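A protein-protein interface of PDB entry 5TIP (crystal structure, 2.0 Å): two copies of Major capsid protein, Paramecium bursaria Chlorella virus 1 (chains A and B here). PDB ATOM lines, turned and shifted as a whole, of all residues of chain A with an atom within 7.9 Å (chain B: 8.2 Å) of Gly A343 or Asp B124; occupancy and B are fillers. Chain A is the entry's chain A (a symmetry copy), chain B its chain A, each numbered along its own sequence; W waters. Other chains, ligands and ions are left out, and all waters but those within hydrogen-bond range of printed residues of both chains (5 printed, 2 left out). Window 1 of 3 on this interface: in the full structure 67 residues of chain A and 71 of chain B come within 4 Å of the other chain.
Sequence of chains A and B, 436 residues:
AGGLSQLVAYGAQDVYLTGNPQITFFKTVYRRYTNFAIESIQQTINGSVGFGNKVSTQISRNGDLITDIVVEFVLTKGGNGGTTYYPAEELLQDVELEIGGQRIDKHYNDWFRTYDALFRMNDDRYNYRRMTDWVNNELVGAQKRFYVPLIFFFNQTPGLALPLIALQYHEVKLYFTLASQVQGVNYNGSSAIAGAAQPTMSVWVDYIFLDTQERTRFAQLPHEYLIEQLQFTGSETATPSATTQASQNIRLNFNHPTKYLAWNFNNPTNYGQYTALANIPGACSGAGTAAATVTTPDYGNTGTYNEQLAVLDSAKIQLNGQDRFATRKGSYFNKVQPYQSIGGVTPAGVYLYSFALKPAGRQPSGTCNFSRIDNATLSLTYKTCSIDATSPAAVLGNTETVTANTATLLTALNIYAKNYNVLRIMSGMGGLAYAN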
ATOM      1  N   LEU A 118      19.064  22.669 -12.297  1.00  0.00           N
ATOM      2  CA  LEU A 118      19.564  23.299 -13.512  1.00  0.00           C
ATOM      3  C   LEU A 118      19.832  24.792 -13.365  1.00  0.00           C
ATOM      4  O   LEU A 118      20.868  25.272 -13.832  1.00  0.00           O
ATOM      5  CB  LEU A 118      18.577  23.081 -14.665  1.00  0.00           C
ATOM      6  CG  LEU A 118      18.626  21.737 -15.392  1.00  0.00           C
ATOM      7  CD1 LEU A 118      17.473  21.636 -16.372  1.00  0.00           C
ATOM      8  CD2 LEU A 118      19.954  21.562 -16.113  1.00  0.00           C
ATOM      9  N   ARG A 120      19.401  26.954 -10.398  1.00  0.00           N
ATOM     10  CA  ARG A 120      19.975  27.512  -9.184  1.00  0.00           C
ATOM     11  C   ARG A 120      21.408  27.025  -9.029  1.00  0.00           C
ATOM     12  O   ARG A 120      21.798  25.986  -9.566  1.00  0.00           O
ATOM     13  CB  ARG A 120      19.145  27.144  -7.953  1.00  0.00           C
ATOM     14  CG  ARG A 120      17.900  28.001  -7.787  1.00  0.00           C
ATOM     15  CD  ARG A 120      17.366  27.950  -6.364  1.00  0.00           C
ATOM     16  NE  ARG A 120      16.028  28.527  -6.270  1.00  0.00           N
ATOM     17  CZ  ARG A 120      14.909  27.851  -6.504  1.00  0.00           C
ATOM     18  NH1 ARG A 120      14.965  26.572  -6.844  1.00  0.00           N
ATOM     19  NH2 ARG A 120      13.733  28.453  -6.399  1.00  0.00           N
ATOM     20  N   MET A 121      22.197  27.797  -8.288  1.00  0.00           N
ATOM     21  CA  MET A 121      23.612  27.490  -8.153  1.00  0.00           C
ATOM     22  C   MET A 121      24.172  28.207  -6.937  1.00  0.00           C
ATOM     23  O   MET A 121      23.585  29.167  -6.432  1.00  0.00           O
ATOM     24  CB  MET A 121      24.396  27.897  -9.405  1.00  0.00           C
ATOM     25  CG  MET A 121      24.404  29.398  -9.651  1.00  0.00           C
ATOM     26  SD  MET A 121      25.198  29.877 -11.198  1.00  0.00           S
ATOM     27  CE  MET A 121      24.042  29.217 -12.395  1.00  0.00           C
ATOM     28  N   ASN A 122      25.314  27.711  -6.476  1.00  0.00           N
ATOM     29  CA  ASN A 122      26.192  28.410  -5.521  1.00  0.00           C
ATOM     30  C   ASN A 122      25.442  28.578  -4.194  1.00  0.00           C
ATOM     31  O   ASN A 122      24.673  27.685  -3.806  1.00  0.00           O
ATOM     32  CB  ASN A 122      26.678  29.695  -6.154  1.00  0.00           C
ATOM     33  CG  ASN A 122      27.471  29.453  -7.417  1.00  0.00           C
ATOM     34  OD1 ASN A 122      28.187  28.459  -7.527  1.00  0.00           O
ATOM     35  ND2 ASN A 122      27.349  30.358  -8.380  1.00  0.00           N
ATOM     36  N   ARG A 125      21.574  28.379  -4.131  1.00  0.00           N
ATOM     37  CA  ARG A 125      21.065  27.017  -4.132  1.00  0.00           C
ATOM     38  C   ARG A 125      21.059  26.449  -2.714  1.00  0.00           C
ATOM     39  O   ARG A 125      20.091  25.807  -2.307  1.00  0.00           O
ATOM     40  CB  ARG A 125      21.905  26.130  -5.053  1.00  0.00           C
ATOM     41  CG  ARG A 125      21.353  24.726  -5.236  1.00  0.00           C
ATOM     42  CD  ARG A 125      21.434  24.286  -6.689  1.00  0.00           C
ATOM     43  NE  ARG A 125      22.787  23.886  -7.064  1.00  0.00           N
ATOM     44  CZ  ARG A 125      23.113  23.371  -8.245  1.00  0.00           C
ATOM     45  NH1 ARG A 125      22.182  23.191  -9.172  1.00  0.00           N
ATOM     46  NH2 ARG A 125      24.370  23.036  -8.500  1.00  0.00           N
ATOM     47  N   LYS A 335      26.541  18.148 -18.741  1.00  0.00           N
ATOM     48  CA  LYS A 335      27.693  18.994 -18.460  1.00  0.00           C
ATOM     49  C   LYS A 335      27.844  20.150 -19.435  1.00  0.00           C
ATOM     50  O   LYS A 335      28.001  21.300 -19.011  1.00  0.00           O
ATOM     51  CB  LYS A 335      28.967  18.139 -18.481  1.00  0.00           C
ATOM     52  CG  LYS A 335      29.030  17.093 -17.389  1.00  0.00           C
ATOM     53  CD  LYS A 335      30.316  16.299 -17.488  1.00  0.00           C
ATOM     54  CE  LYS A 335      30.414  15.275 -16.378  1.00  0.00           C
ATOM     55  NZ  LYS A 335      31.251  14.119 -16.796  1.00  0.00           N
ATOM     56  N   VAL A 336      27.795  19.876 -20.740  1.00  0.00           N
ATOM     57  CA  VAL A 336      28.188  20.871 -21.733  1.00  0.00           C
ATOM     58  C   VAL A 336      27.055  21.847 -22.009  1.00  0.00           C
ATOM     59  O   VAL A 336      27.264  23.065 -22.047  1.00  0.00           O
ATOM     60  CB  VAL A 336      28.655  20.176 -23.021  1.00  0.00           C
ATOM     61  CG1 VAL A 336      29.091  21.207 -24.051  1.00  0.00           C
ATOM     62  CG2 VAL A 336      29.776  19.225 -22.706  1.00  0.00           C
ATOM     63  N   GLN A 337      25.847  21.330 -22.235  1.00  0.00           N
ATOM     64  CA  GLN A 337      24.702  22.217 -22.432  1.00  0.00           C
ATOM     65  C   GLN A 337      24.504  23.165 -21.258  1.00  0.00           C
ATOM     66  O   GLN A 337      24.262  24.361 -21.496  1.00  0.00           O
ATOM     67  CB  GLN A 337      23.445  21.388 -22.711  1.00  0.00           C
ATOM     68  CG  GLN A 337      23.313  20.928 -24.148  1.00  0.00           C
ATOM     69  CD  GLN A 337      22.835  22.031 -25.064  1.00  0.00           C
ATOM     70  OE1 GLN A 337      22.070  22.905 -24.656  1.00  0.00           O
ATOM     71  NE2 GLN A 337      23.280  21.995 -26.314  1.00  0.00           N
ATOM     72  N   PRO A 338      24.582  22.727 -19.995  1.00  0.00           N
ATOM     73  CA  PRO A 338      24.535  23.714 -18.904  1.00  0.00           C
ATOM     74  C   PRO A 338      25.754  24.621 -18.859  1.00  0.00           C
ATOM     75  O   PRO A 338      25.620  25.807 -18.534  1.00  0.00           O
ATOM     76  CB  PRO A 338      24.424  22.838 -17.648  1.00  0.00           C
ATOM     77  CG  PRO A 338      23.858  21.552 -18.132  1.00  0.00           C
ATOM     78  CD  PRO A 338      24.482  21.353 -19.473  1.00  0.00           C
ATOM     79  N   TYR A 339      26.946  24.104 -19.178  1.00  0.00           N
ATOM     80  CA  TYR A 339      28.136  24.951 -19.175  1.00  0.00           C
ATOM     81  C   TYR A 339      28.017  26.079 -20.191  1.00  0.00           C
ATOM     82  O   TYR A 339      28.406  27.219 -19.912  1.00  0.00           O
ATOM     83  CB  TYR A 339      29.387  24.115 -19.460  1.00  0.00           C
ATOM     84  CG  TYR A 339      30.658  24.936 -19.596  1.00  0.00           C
ATOM     85  CD1 TYR A 339      31.417  25.270 -18.481  1.00  0.00           C
ATOM     86  CD2 TYR A 339      31.094  25.376 -20.839  1.00  0.00           C
ATOM     87  CE1 TYR A 339      32.573  26.023 -18.603  1.00  0.00           C
ATOM     88  CE2 TYR A 339      32.247  26.129 -20.969  1.00  0.00           C
ATOM     89  CZ  TYR A 339      32.983  26.449 -19.848  1.00  0.00           C
ATOM     90  OH  TYR A 339      34.132  27.197 -19.974  1.00  0.00           O
ATOM     91  N   GLN A 340      27.472  25.784 -21.371  1.00  0.00           N
ATOM     92  CA  GLN A 340      27.430  26.763 -22.449  1.00  0.00           C
ATOM     93  C   GLN A 340      26.316  27.790 -22.290  1.00  0.00           C
ATOM     94  O   GLN A 340      26.412  28.875 -22.870  1.00  0.00           O
ATOM     95  CB  GLN A 340      27.278  26.056 -23.798  1.00  0.00           C
ATOM     96  CG  GLN A 340      28.506  25.276 -24.231  1.00  0.00           C
ATOM     97  CD  GLN A 340      28.309  24.572 -25.557  1.00  0.00           C
ATOM     98  OE1 GLN A 340      27.179  24.329 -25.983  1.00  0.00           O
ATOM     99  NE2 GLN A 340      29.411  24.240 -26.219  1.00  0.00           N
ATOM    100  N   SER A 341      25.271  27.486 -21.520  1.00  0.00           N
ATOM    101  CA  SER A 341      24.091  28.338 -21.488  1.00  0.00           C
ATOM    102  C   SER A 341      23.634  28.756 -20.097  1.00  0.00           C
ATOM    103  O   SER A 341      22.812  29.673 -19.998  1.00  0.00           O
ATOM    104  CB  SER A 341      22.918  27.647 -22.202  1.00  0.00           C
ATOM    105  OG  SER A 341      22.562  26.440 -21.550  1.00  0.00           O
ATOM    106  N   ILE A 342      24.135  28.136 -19.028  1.00  0.00           N
ATOM    107  CA  ILE A 342      23.712  28.439 -17.666  1.00  0.00           C
ATOM    108  C   ILE A 342      24.872  28.953 -16.821  1.00  0.00           C
ATOM    109  O   ILE A 342      24.794  30.037 -16.234  1.00  0.00           O
ATOM    110  CB  ILE A 342      23.050  27.213 -16.994  1.00  0.00           C
ATOM    111  CG1 ILE A 342      21.788  26.801 -17.754  1.00  0.00           C
ATOM    112  CG2 ILE A 342      22.716  27.519 -15.544  1.00  0.00           C
ATOM    113  CD1 ILE A 342      21.101  25.581 -17.177  1.00  0.00           C
ATOM    114  N   GLY A 343      25.956  28.188 -16.747  1.00  0.00           N
ATOM    115  CA  GLY A 343      27.109  28.593 -15.970  1.00  0.00           C
ATOM    116  C   GLY A 343      27.096  28.150 -14.527  1.00  0.00           C
ATOM    117  O   GLY A 343      27.671  28.836 -13.674  1.00  0.00           O
ATOM    118  N   GLY A 344      26.453  27.028 -14.220  1.00  0.00           N
ATOM    119  CA  GLY A 344      26.481  26.469 -12.882  1.00  0.00           C
ATOM    120  C   GLY A 344      27.019  25.054 -12.894  1.00  0.00           C
ATOM    121  O   GLY A 344      27.979  24.758 -13.610  1.00  0.00           O
ATOM    122  N   VAL A 345      26.411  24.169 -12.110  1.00  0.00           N
ATOM    123  CA  VAL A 345      26.732  22.746 -12.143  1.00  0.00           C
ATOM    124  C   VAL A 345      25.437  21.969 -11.945  1.00  0.00           C
ATOM    125  O   VAL A 345      24.618  22.319 -11.088  1.00  0.00           O
ATOM    126  CB  VAL A 345      27.796  22.352 -11.096  1.00  0.00           C
ATOM    127  CG1 VAL A 345      27.267  22.493  -9.676  1.00  0.00           C
ATOM    128  CG2 VAL A 345      28.289  20.936 -11.349  1.00  0.00           C
ATOM    129  N   THR A 346      25.234  20.942 -12.761  1.00  0.00           N
ATOM    130  CA  THR A 346      24.008  20.171 -12.745  1.00  0.00           C
ATOM    131  C   THR A 346      24.305  18.744 -12.311  1.00  0.00           C
ATOM    132  O   THR A 346      25.192  18.099 -12.889  1.00  0.00           O
ATOM    133  CB  THR A 346      23.341  20.169 -14.129  1.00  0.00           C
ATOM    134  OG1 THR A 346      22.936  21.502 -14.464  1.00  0.00           O
ATOM    135  CG2 THR A 346      22.122  19.265 -14.132  1.00  0.00           C
ATOM    136  N   PRO A 359      18.936  30.605 -21.511  1.00  0.00           N
ATOM    137  CA  PRO A 359      17.634  30.060 -21.093  1.00  0.00           C
ATOM    138  C   PRO A 359      17.171  30.548 -19.731  1.00  0.00           C
ATOM    139  O   PRO A 359      15.960  30.584 -19.480  1.00  0.00           O
ATOM    140  CB  PRO A 359      17.877  28.543 -21.094  1.00  0.00           C
ATOM    141  CG  PRO A 359      19.349  28.397 -20.916  1.00  0.00           C
ATOM    142  CD  PRO A 359      19.959  29.556 -21.644  1.00  0.00           C
ATOM    143  N   ALA A 360      18.091  30.929 -18.846  1.00  0.00           N
ATOM    144  CA  ALA A 360      17.707  31.420 -17.528  1.00  0.00           C
ATOM    145  C   ALA A 360      17.327  32.893 -17.526  1.00  0.00           C
ATOM    146  O   ALA A 360      16.875  33.395 -16.491  1.00  0.00           O
ATOM    147  CB  ALA A 360      18.838  31.182 -16.525  1.00  0.00           C
ATOM    148  N   TYR B 115      43.802  30.549 -16.833  1.00  0.00           N
ATOM    149  CA  TYR B 115      42.490  31.159 -17.025  1.00  0.00           C
ATOM    150  C   TYR B 115      41.472  30.592 -16.045  1.00  0.00           C
ATOM    151  O   TYR B 115      40.640  31.331 -15.505  1.00  0.00           O
ATOM    152  CB  TYR B 115      42.024  30.950 -18.466  1.00  0.00           C
ATOM    153  CG  TYR B 115      40.615  31.424 -18.736  1.00  0.00           C
ATOM    154  CD1 TYR B 115      40.361  32.740 -19.087  1.00  0.00           C
ATOM    155  CD2 TYR B 115      39.539  30.551 -18.644  1.00  0.00           C
ATOM    156  CE1 TYR B 115      39.076  33.177 -19.334  1.00  0.00           C
ATOM    157  CE2 TYR B 115      38.250  30.978 -18.889  1.00  0.00           C
ATOM    158  CZ  TYR B 115      38.025  32.292 -19.235  1.00  0.00           C
ATOM    159  OH  TYR B 115      36.743  32.729 -19.484  1.00  0.00           O
ATOM    160  N   ASP B 116      41.521  29.281 -15.805  1.00  0.00           N
ATOM    161  CA  ASP B 116      40.578  28.660 -14.882  1.00  0.00           C
ATOM    162  C   ASP B 116      40.792  29.153 -13.456  1.00  0.00           C
ATOM    163  O   ASP B 116      39.826  29.348 -12.709  1.00  0.00           O
ATOM    164  CB  ASP B 116      40.710  27.138 -14.956  1.00  0.00           C
ATOM    165  CG  ASP B 116      39.666  26.419 -14.125  1.00  0.00           C
ATOM    166  OD1 ASP B 116      38.460  26.627 -14.373  1.00  0.00           O
ATOM    167  OD2 ASP B 116      40.050  25.641 -13.227  1.00  0.00           O
ATOM    168  N   PHE B 119      39.605  33.340 -13.791  1.00  0.00           N
ATOM    169  CA  PHE B 119      38.371  33.871 -14.352  1.00  0.00           C
ATOM    170  C   PHE B 119      37.186  32.917 -14.270  1.00  0.00           C
ATOM    171  O   PHE B 119      36.073  33.307 -14.638  1.00  0.00           O
ATOM    172  CB  PHE B 119      38.609  34.297 -15.804  1.00  0.00           C
ATOM    173  CG  PHE B 119      39.630  35.386 -15.939  1.00  0.00           C
ATOM    174  CD1 PHE B 119      39.306  36.695 -15.628  1.00  0.00           C
ATOM    175  CD2 PHE B 119      40.921  35.099 -16.351  1.00  0.00           C
ATOM    176  CE1 PHE B 119      40.244  37.700 -15.738  1.00  0.00           C
ATOM    177  CE2 PHE B 119      41.865  36.101 -16.463  1.00  0.00           C
ATOM    178  CZ  PHE B 119      41.526  37.403 -16.155  1.00  0.00           C
ATOM    179  N   ARG B 120      37.384  31.688 -13.813  1.00  0.00           N
ATOM    180  CA  ARG B 120      36.263  30.833 -13.453  1.00  0.00           C
ATOM    181  C   ARG B 120      36.116  30.801 -11.938  1.00  0.00           C
ATOM    182  O   ARG B 120      37.065  31.051 -11.193  1.00  0.00           O
ATOM    183  CB  ARG B 120      36.438  29.418 -14.008  1.00  0.00           C
ATOM    184  CG  ARG B 120      36.084  29.301 -15.482  1.00  0.00           C
ATOM    185  CD  ARG B 120      35.810  27.861 -15.883  1.00  0.00           C
ATOM    186  NE  ARG B 120      35.758  27.706 -17.333  1.00  0.00           N
ATOM    187  CZ  ARG B 120      36.825  27.509 -18.100  1.00  0.00           C
ATOM    188  NH1 ARG B 120      38.030  27.440 -17.554  1.00  0.00           N
ATOM    189  NH2 ARG B 120      36.688  27.382 -19.412  1.00  0.00           N
ATOM    190  N   MET B 121      34.903  30.494 -11.489  1.00  0.00           N
ATOM    191  CA  MET B 121      34.614  30.533 -10.064  1.00  0.00           C
ATOM    192  C   MET B 121      33.361  29.723  -9.780  1.00  0.00           C
ATOM    193  O   MET B 121      32.561  29.442 -10.677  1.00  0.00           O
ATOM    194  CB  MET B 121      34.429  31.971  -9.569  1.00  0.00           C
ATOM    195  CG  MET B 121      33.218  32.667 -10.172  1.00  0.00           C
ATOM    196  SD  MET B 121      33.074  34.404  -9.709  1.00  0.00           S
ATOM    197  CE  MET B 121      34.485  35.104 -10.561  1.00  0.00           C
ATOM    198  N   ASN B 122      33.216  29.348  -8.515  1.00  0.00           N
ATOM    199  CA  ASN B 122      31.958  28.836  -7.944  1.00  0.00           C
ATOM    200  C   ASN B 122      31.607  27.513  -8.635  1.00  0.00           C
ATOM    201  O   ASN B 122      32.514  26.732  -8.964  1.00  0.00           O
ATOM    202  CB  ASN B 122      30.901  29.914  -8.042  1.00  0.00           C
ATOM    203  CG  ASN B 122      31.278  31.162  -7.279  1.00  0.00           C
ATOM    204  OD1 ASN B 122      31.918  31.088  -6.233  1.00  0.00           O
ATOM    205  ND2 ASN B 122      30.883  32.319  -7.798  1.00  0.00           N
ATOM    206  N   ASP B 123      30.315  27.235  -8.849  1.00  0.00           N
ATOM    207  CA  ASP B 123      29.893  25.962  -9.429  1.00  0.00           C
ATOM    208  C   ASP B 123      30.319  25.833 -10.885  1.00  0.00           C
ATOM    209  O   ASP B 123      30.545  24.716 -11.364  1.00  0.00           O
ATOM    210  CB  ASP B 123      28.378  25.815  -9.313  1.00  0.00           C
ATOM    211  CG  ASP B 123      27.930  25.531  -7.898  1.00  0.00           C
ATOM    212  OD1 ASP B 123      28.795  25.325  -7.021  1.00  0.00           O
ATOM    213  OD2 ASP B 123      26.706  25.530  -7.662  1.00  0.00           O
ATOM    214  N   ASP B 124      30.432  26.957 -11.597  1.00  0.00           N
ATOM    215  CA  ASP B 124      30.905  26.925 -12.974  1.00  0.00           C
ATOM    216  C   ASP B 124      32.301  26.328 -13.063  1.00  0.00           C
ATOM    217  O   ASP B 124      32.581  25.502 -13.946  1.00  0.00           O
ATOM    218  CB  ASP B 124      30.891  28.339 -13.543  1.00  0.00           C
ATOM    219  CG  ASP B 124      31.287  28.383 -14.993  1.00  0.00           C
ATOM    220  OD1 ASP B 124      30.780  27.578 -15.794  1.00  0.00           O
ATOM    221  OD2 ASP B 124      32.113  29.230 -15.353  1.00  0.00           O
ATOM    222  N   ARG B 125      33.138  26.683 -12.094  1.00  0.00           N
ATOM    223  CA  ARG B 125      34.496  26.167 -12.017  1.00  0.00           C
ATOM    224  C   ARG B 125      34.482  24.668 -11.729  1.00  0.00           C
ATOM    225  O   ARG B 125      35.237  23.911 -12.339  1.00  0.00           O
ATOM    226  CB  ARG B 125      35.290  26.906 -10.938  1.00  0.00           C
ATOM    227  CG  ARG B 125      36.764  26.540 -10.892  1.00  0.00           C
ATOM    228  CD  ARG B 125      37.634  27.773 -10.711  1.00  0.00           C
ATOM    229  NE  ARG B 125      37.629  28.248  -9.330  1.00  0.00           N
ATOM    230  CZ  ARG B 125      38.379  29.249  -8.883  1.00  0.00           C
ATOM    231  NH1 ARG B 125      39.198  29.888  -9.707  1.00  0.00           N
ATOM    232  NH2 ARG B 125      38.310  29.614  -7.610  1.00  0.00           N
ATOM    233  N   TYR B 126      33.628  24.233 -10.802  1.00  0.00           N
ATOM    234  CA  TYR B 126      33.555  22.813 -10.478  1.00  0.00           C
ATOM    235  C   TYR B 126      33.005  22.003 -11.645  1.00  0.00           C
ATOM    236  O   TYR B 126      33.456  20.876 -11.893  1.00  0.00           O
ATOM    237  CB  TYR B 126      32.699  22.593  -9.230  1.00  0.00           C
ATOM    238  CG  TYR B 126      32.515  21.127  -8.879  1.00  0.00           C
ATOM    239  CD1 TYR B 126      33.593  20.345  -8.517  1.00  0.00           C
ATOM    240  CD2 TYR B 126      31.262  20.534  -8.879  1.00  0.00           C
ATOM    241  CE1 TYR B 126      33.448  19.009  -8.195  1.00  0.00           C
ATOM    242  CE2 TYR B 126      31.104  19.191  -8.548  1.00  0.00           C
ATOM    243  CZ  TYR B 126      32.202  18.440  -8.210  1.00  0.00           C
ATOM    244  OH  TYR B 126      32.061  17.110  -7.881  1.00  0.00           O
ATOM    245  N   ASN B 127      32.017  22.553 -12.366  1.00  0.00           N
ATOM    246  CA  ASN B 127      31.526  21.871 -13.563  1.00  0.00           C
ATOM    247  C   ASN B 127      32.619  21.726 -14.614  1.00  0.00           C
ATOM    248  O   ASN B 127      32.650  20.733 -15.347  1.00  0.00           O
ATOM    249  CB  ASN B 127      30.330  22.627 -14.150  1.00  0.00           C
ATOM    250  CG  ASN B 127      29.625  21.849 -15.255  1.00  0.00           C
ATOM    251  OD1 ASN B 127      29.491  20.631 -15.175  1.00  0.00           O
ATOM    252  ND2 ASN B 127      29.178  22.556 -16.296  1.00  0.00           N
ATOM    253  N   TYR B 128      33.518  22.710 -14.698  1.00  0.00           N
ATOM    254  CA  TYR B 128      34.634  22.604 -15.628  1.00  0.00           C
ATOM    255  C   TYR B 128      35.575  21.470 -15.247  1.00  0.00           C
ATOM    256  O   TYR B 128      36.143  20.819 -16.130  1.00  0.00           O
ATOM    257  CB  TYR B 128      35.393  23.934 -15.697  1.00  0.00           C
ATOM    258  CG  TYR B 128      36.646  23.889 -16.548  1.00  0.00           C
ATOM    259  CD1 TYR B 128      36.573  23.998 -17.930  1.00  0.00           C
ATOM    260  CD2 TYR B 128      37.901  23.753 -15.967  1.00  0.00           C
ATOM    261  CE1 TYR B 128      37.714  23.962 -18.711  1.00  0.00           C
ATOM    262  CE2 TYR B 128      39.047  23.716 -16.742  1.00  0.00           C
ATOM    263  CZ  TYR B 128      38.947  23.822 -18.113  1.00  0.00           C
ATOM    264  OH  TYR B 128      40.086  23.788 -18.883  1.00  0.00           O
ATOM    265  N   ARG B 129      35.752  21.209 -13.946  1.00  0.00           N
ATOM    266  CA  ARG B 129      36.595  20.085 -13.552  1.00  0.00           C
ATOM    267  C   ARG B 129      35.896  18.751 -13.779  1.00  0.00           C
ATOM    268  O   ARG B 129      36.561  17.744 -14.050  1.00  0.00           O
ATOM    269  CB  ARG B 129      37.033  20.208 -12.092  1.00  0.00           C
ATOM    270  CG  ARG B 129      38.095  19.184 -11.730  1.00  0.00           C
ATOM    271  CD  ARG B 129      38.754  19.429 -10.392  1.00  0.00           C
ATOM    272  NE  ARG B 129      39.831  18.464 -10.181  1.00  0.00           N
ATOM    273  CZ  ARG B 129      40.595  18.409  -9.098  1.00  0.00           C
ATOM    274  NH1 ARG B 129      40.412  19.269  -8.107  1.00  0.00           N
ATOM    275  NH2 ARG B 129      41.546  17.489  -9.005  1.00  0.00           N
ATOM    276  N   ARG B 130      34.566  18.713 -13.661  1.00  0.00           N
ATOM    277  CA  ARG B 130      33.835  17.519 -14.071  1.00  0.00           C
ATOM    278  C   ARG B 130      34.080  17.213 -15.541  1.00  0.00           C
ATOM    279  O   ARG B 130      34.159  16.045 -15.936  1.00  0.00           O
ATOM    280  CB  ARG B 130      32.337  17.690 -13.819  1.00  0.00           C
ATOM    281  CG  ARG B 130      31.920  17.810 -12.370  1.00  0.00           C
ATOM    282  CD  ARG B 130      30.420  18.041 -12.297  1.00  0.00           C
ATOM    283  NE  ARG B 130      29.668  16.886 -12.777  1.00  0.00           N
ATOM    284  CZ  ARG B 130      28.436  16.951 -13.271  1.00  0.00           C
ATOM    285  NH1 ARG B 130      27.819  18.119 -13.367  1.00  0.00           N
ATOM    286  NH2 ARG B 130      27.823  15.849 -13.684  1.00  0.00           N
ATOM    287  N   MET B 131      34.201  18.254 -16.366  1.00  0.00           N
ATOM    288  CA  MET B 131      34.373  18.076 -17.799  1.00  0.00           C
ATOM    289  C   MET B 131      35.798  17.711 -18.187  1.00  0.00           C
ATOM    290  O   MET B 131      36.019  17.264 -19.317  1.00  0.00           O
ATOM    291  CB  MET B 131      33.960  19.349 -18.540  1.00  0.00           C
ATOM    292  CG  MET B 131      32.491  19.707 -18.404  1.00  0.00           C
ATOM    293  SD  MET B 131      32.159  21.407 -18.906  1.00  0.00           S
ATOM    294  CE  MET B 131      32.743  21.382 -20.598  1.00  0.00           C
HETATM  295  O   HOH W   1      25.686  24.086  -5.861  1.00  0.00           O
HETATM  296  O   HOH W   2      26.399  20.547 -15.353  1.00  0.00           O
HETATM  297  O   HOH W   3      33.263  29.497 -18.068  1.00  0.00           O
HETATM  298  O   HOH W   4      28.953  25.371 -15.888  1.00  0.00           O
HETATM  299  O   HOH W   5      29.783  28.716 -18.414  1.00  0.00           O
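The side-chain hydroxyl (OH) of Tyr A339 sits at hydrogen-bond distance from the guanidinium group (NH2) of Arg B120 (2.6 Å). The backbone NH of Asp B123 is in hydrogen-bond range of the side-chain amide oxygen of Asn A122 (2.8 Å). OD2 of Asp B123 is in salt-bridge range of NH2 of Arg A125 (3.5 Å). ND2 of Asn B127 is in hydrogen-bond range of O of Lys A335, 3.2 Å away. NH1 of Arg B130 sits at hydrogen-bond distance from O of Thr A346 (2.7 Å). The backbone carbonyl oxygen (O) of Gly A344 sits close to the backbone carbonyl oxygen (O) of Asp B123, 3.4 Å away.
Asn A122 touches its own counterpart, Asn B122. Positions printed for both chains: 120, 121, 122 and 125. Of the 20 pairs that touch across the chains among the printed residues, 1 has its exchanged pair printed and touching as well.
Water W1 lies within hydrogen-bond range of OD2 of Asp B123 (2.5 Å) and NH2 of Arg A125 (3.1 Å). Water W4 lies within hydrogen-bond range of the backbone carbonyl oxygen of Gly A344 (2.6 Å), the side-chain amide nitrogen of Asn B127 (2.9 Å) and the side-chain carboxylate of Asp B124 (2.9 Å). Water W2 lies within hydrogen-bond range of N of Thr A346 (2.9 Å), OD1 of Asn B127 (3.1 Å) and NH1 of Arg B130 (3.4 Å).
Of the 19 printed residues of chain A, 9 touch a printed residue of chain B. Among the printed residues, Asp or Glu carboxylates within 4 Å of a Lys or Arg side-chain nitrogen of the other chain: Arg A125 with Asp B123.
Among the printed residues, pairs that only touch across the chains: Met A121 with Asp B123 (3.7 Å), Asn A122 with Asn B122 (3.1 Å), Lys A335 with Arg B130 (3.6 Å), Lys A335 with Met B131 (3.9 Å), Tyr A339 with Asp B124 (3.6 Å), Tyr A339 with Asn B127 (3.5 Å), Tyr A339 with Met B131 (3.9 Å), Gly A343 with Asp B124 (3.3 Å), Gly A344 with Asp B124 (3.7 Å), Gly A344 with Asn B127 (3.2 Å), Val A345 with Asp B123 (3.5 Å), Val A345 with Tyr B126 (3.9 Å), Val A345 with Asn B127 (3.9 Å) and Val A345 with Arg B130 (3.5 Å).
O of Arg B120 is in hydrogen-bond range of NH1 of Arg B125, 2.8 Å away. The side-chain sulfur of Met B121 sits close to the side-chain amide nitrogen of Asn B122 (3.6 Å). The backbone carbonyl oxygen (O) of Arg A120 is in hydrogen-bond range of the guanidinium group (NH1) of Arg A125 (2.8 Å). ND2 of Asn A122 lies close to SD of Met A121 (3.6 Å).
Of the printed residues of chain B, Met A121 touches Asp B123. Gly A343 touches just one residue of chain B: Asp B124. Of chain B, only Asp B123 (3.4 Å), Asp B124 (3.7 Å) and Asn B127 (3.2 Å) come within 4 Å of Gly A344. Printed residues of chain B within 4 Å of Val A345: Asp B123 (3.5 Å), Tyr B126 (3.9 Å), Asn B127 (3.9 Å) and Arg B130 (3.5 Å). Printed residues of chain A within 4 Å of Asp B123: Met A121 (3.7 Å), Asn A122 (2.8 Å), Arg A125 (3.5 Å), Gly A344 (3.4 Å) and Val A345 (3.5 Å). Asp B124 touches three residues of chain A. The nearest residue of chain B that does not touch Gly A343 is Asp B123 (4.9 Å).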
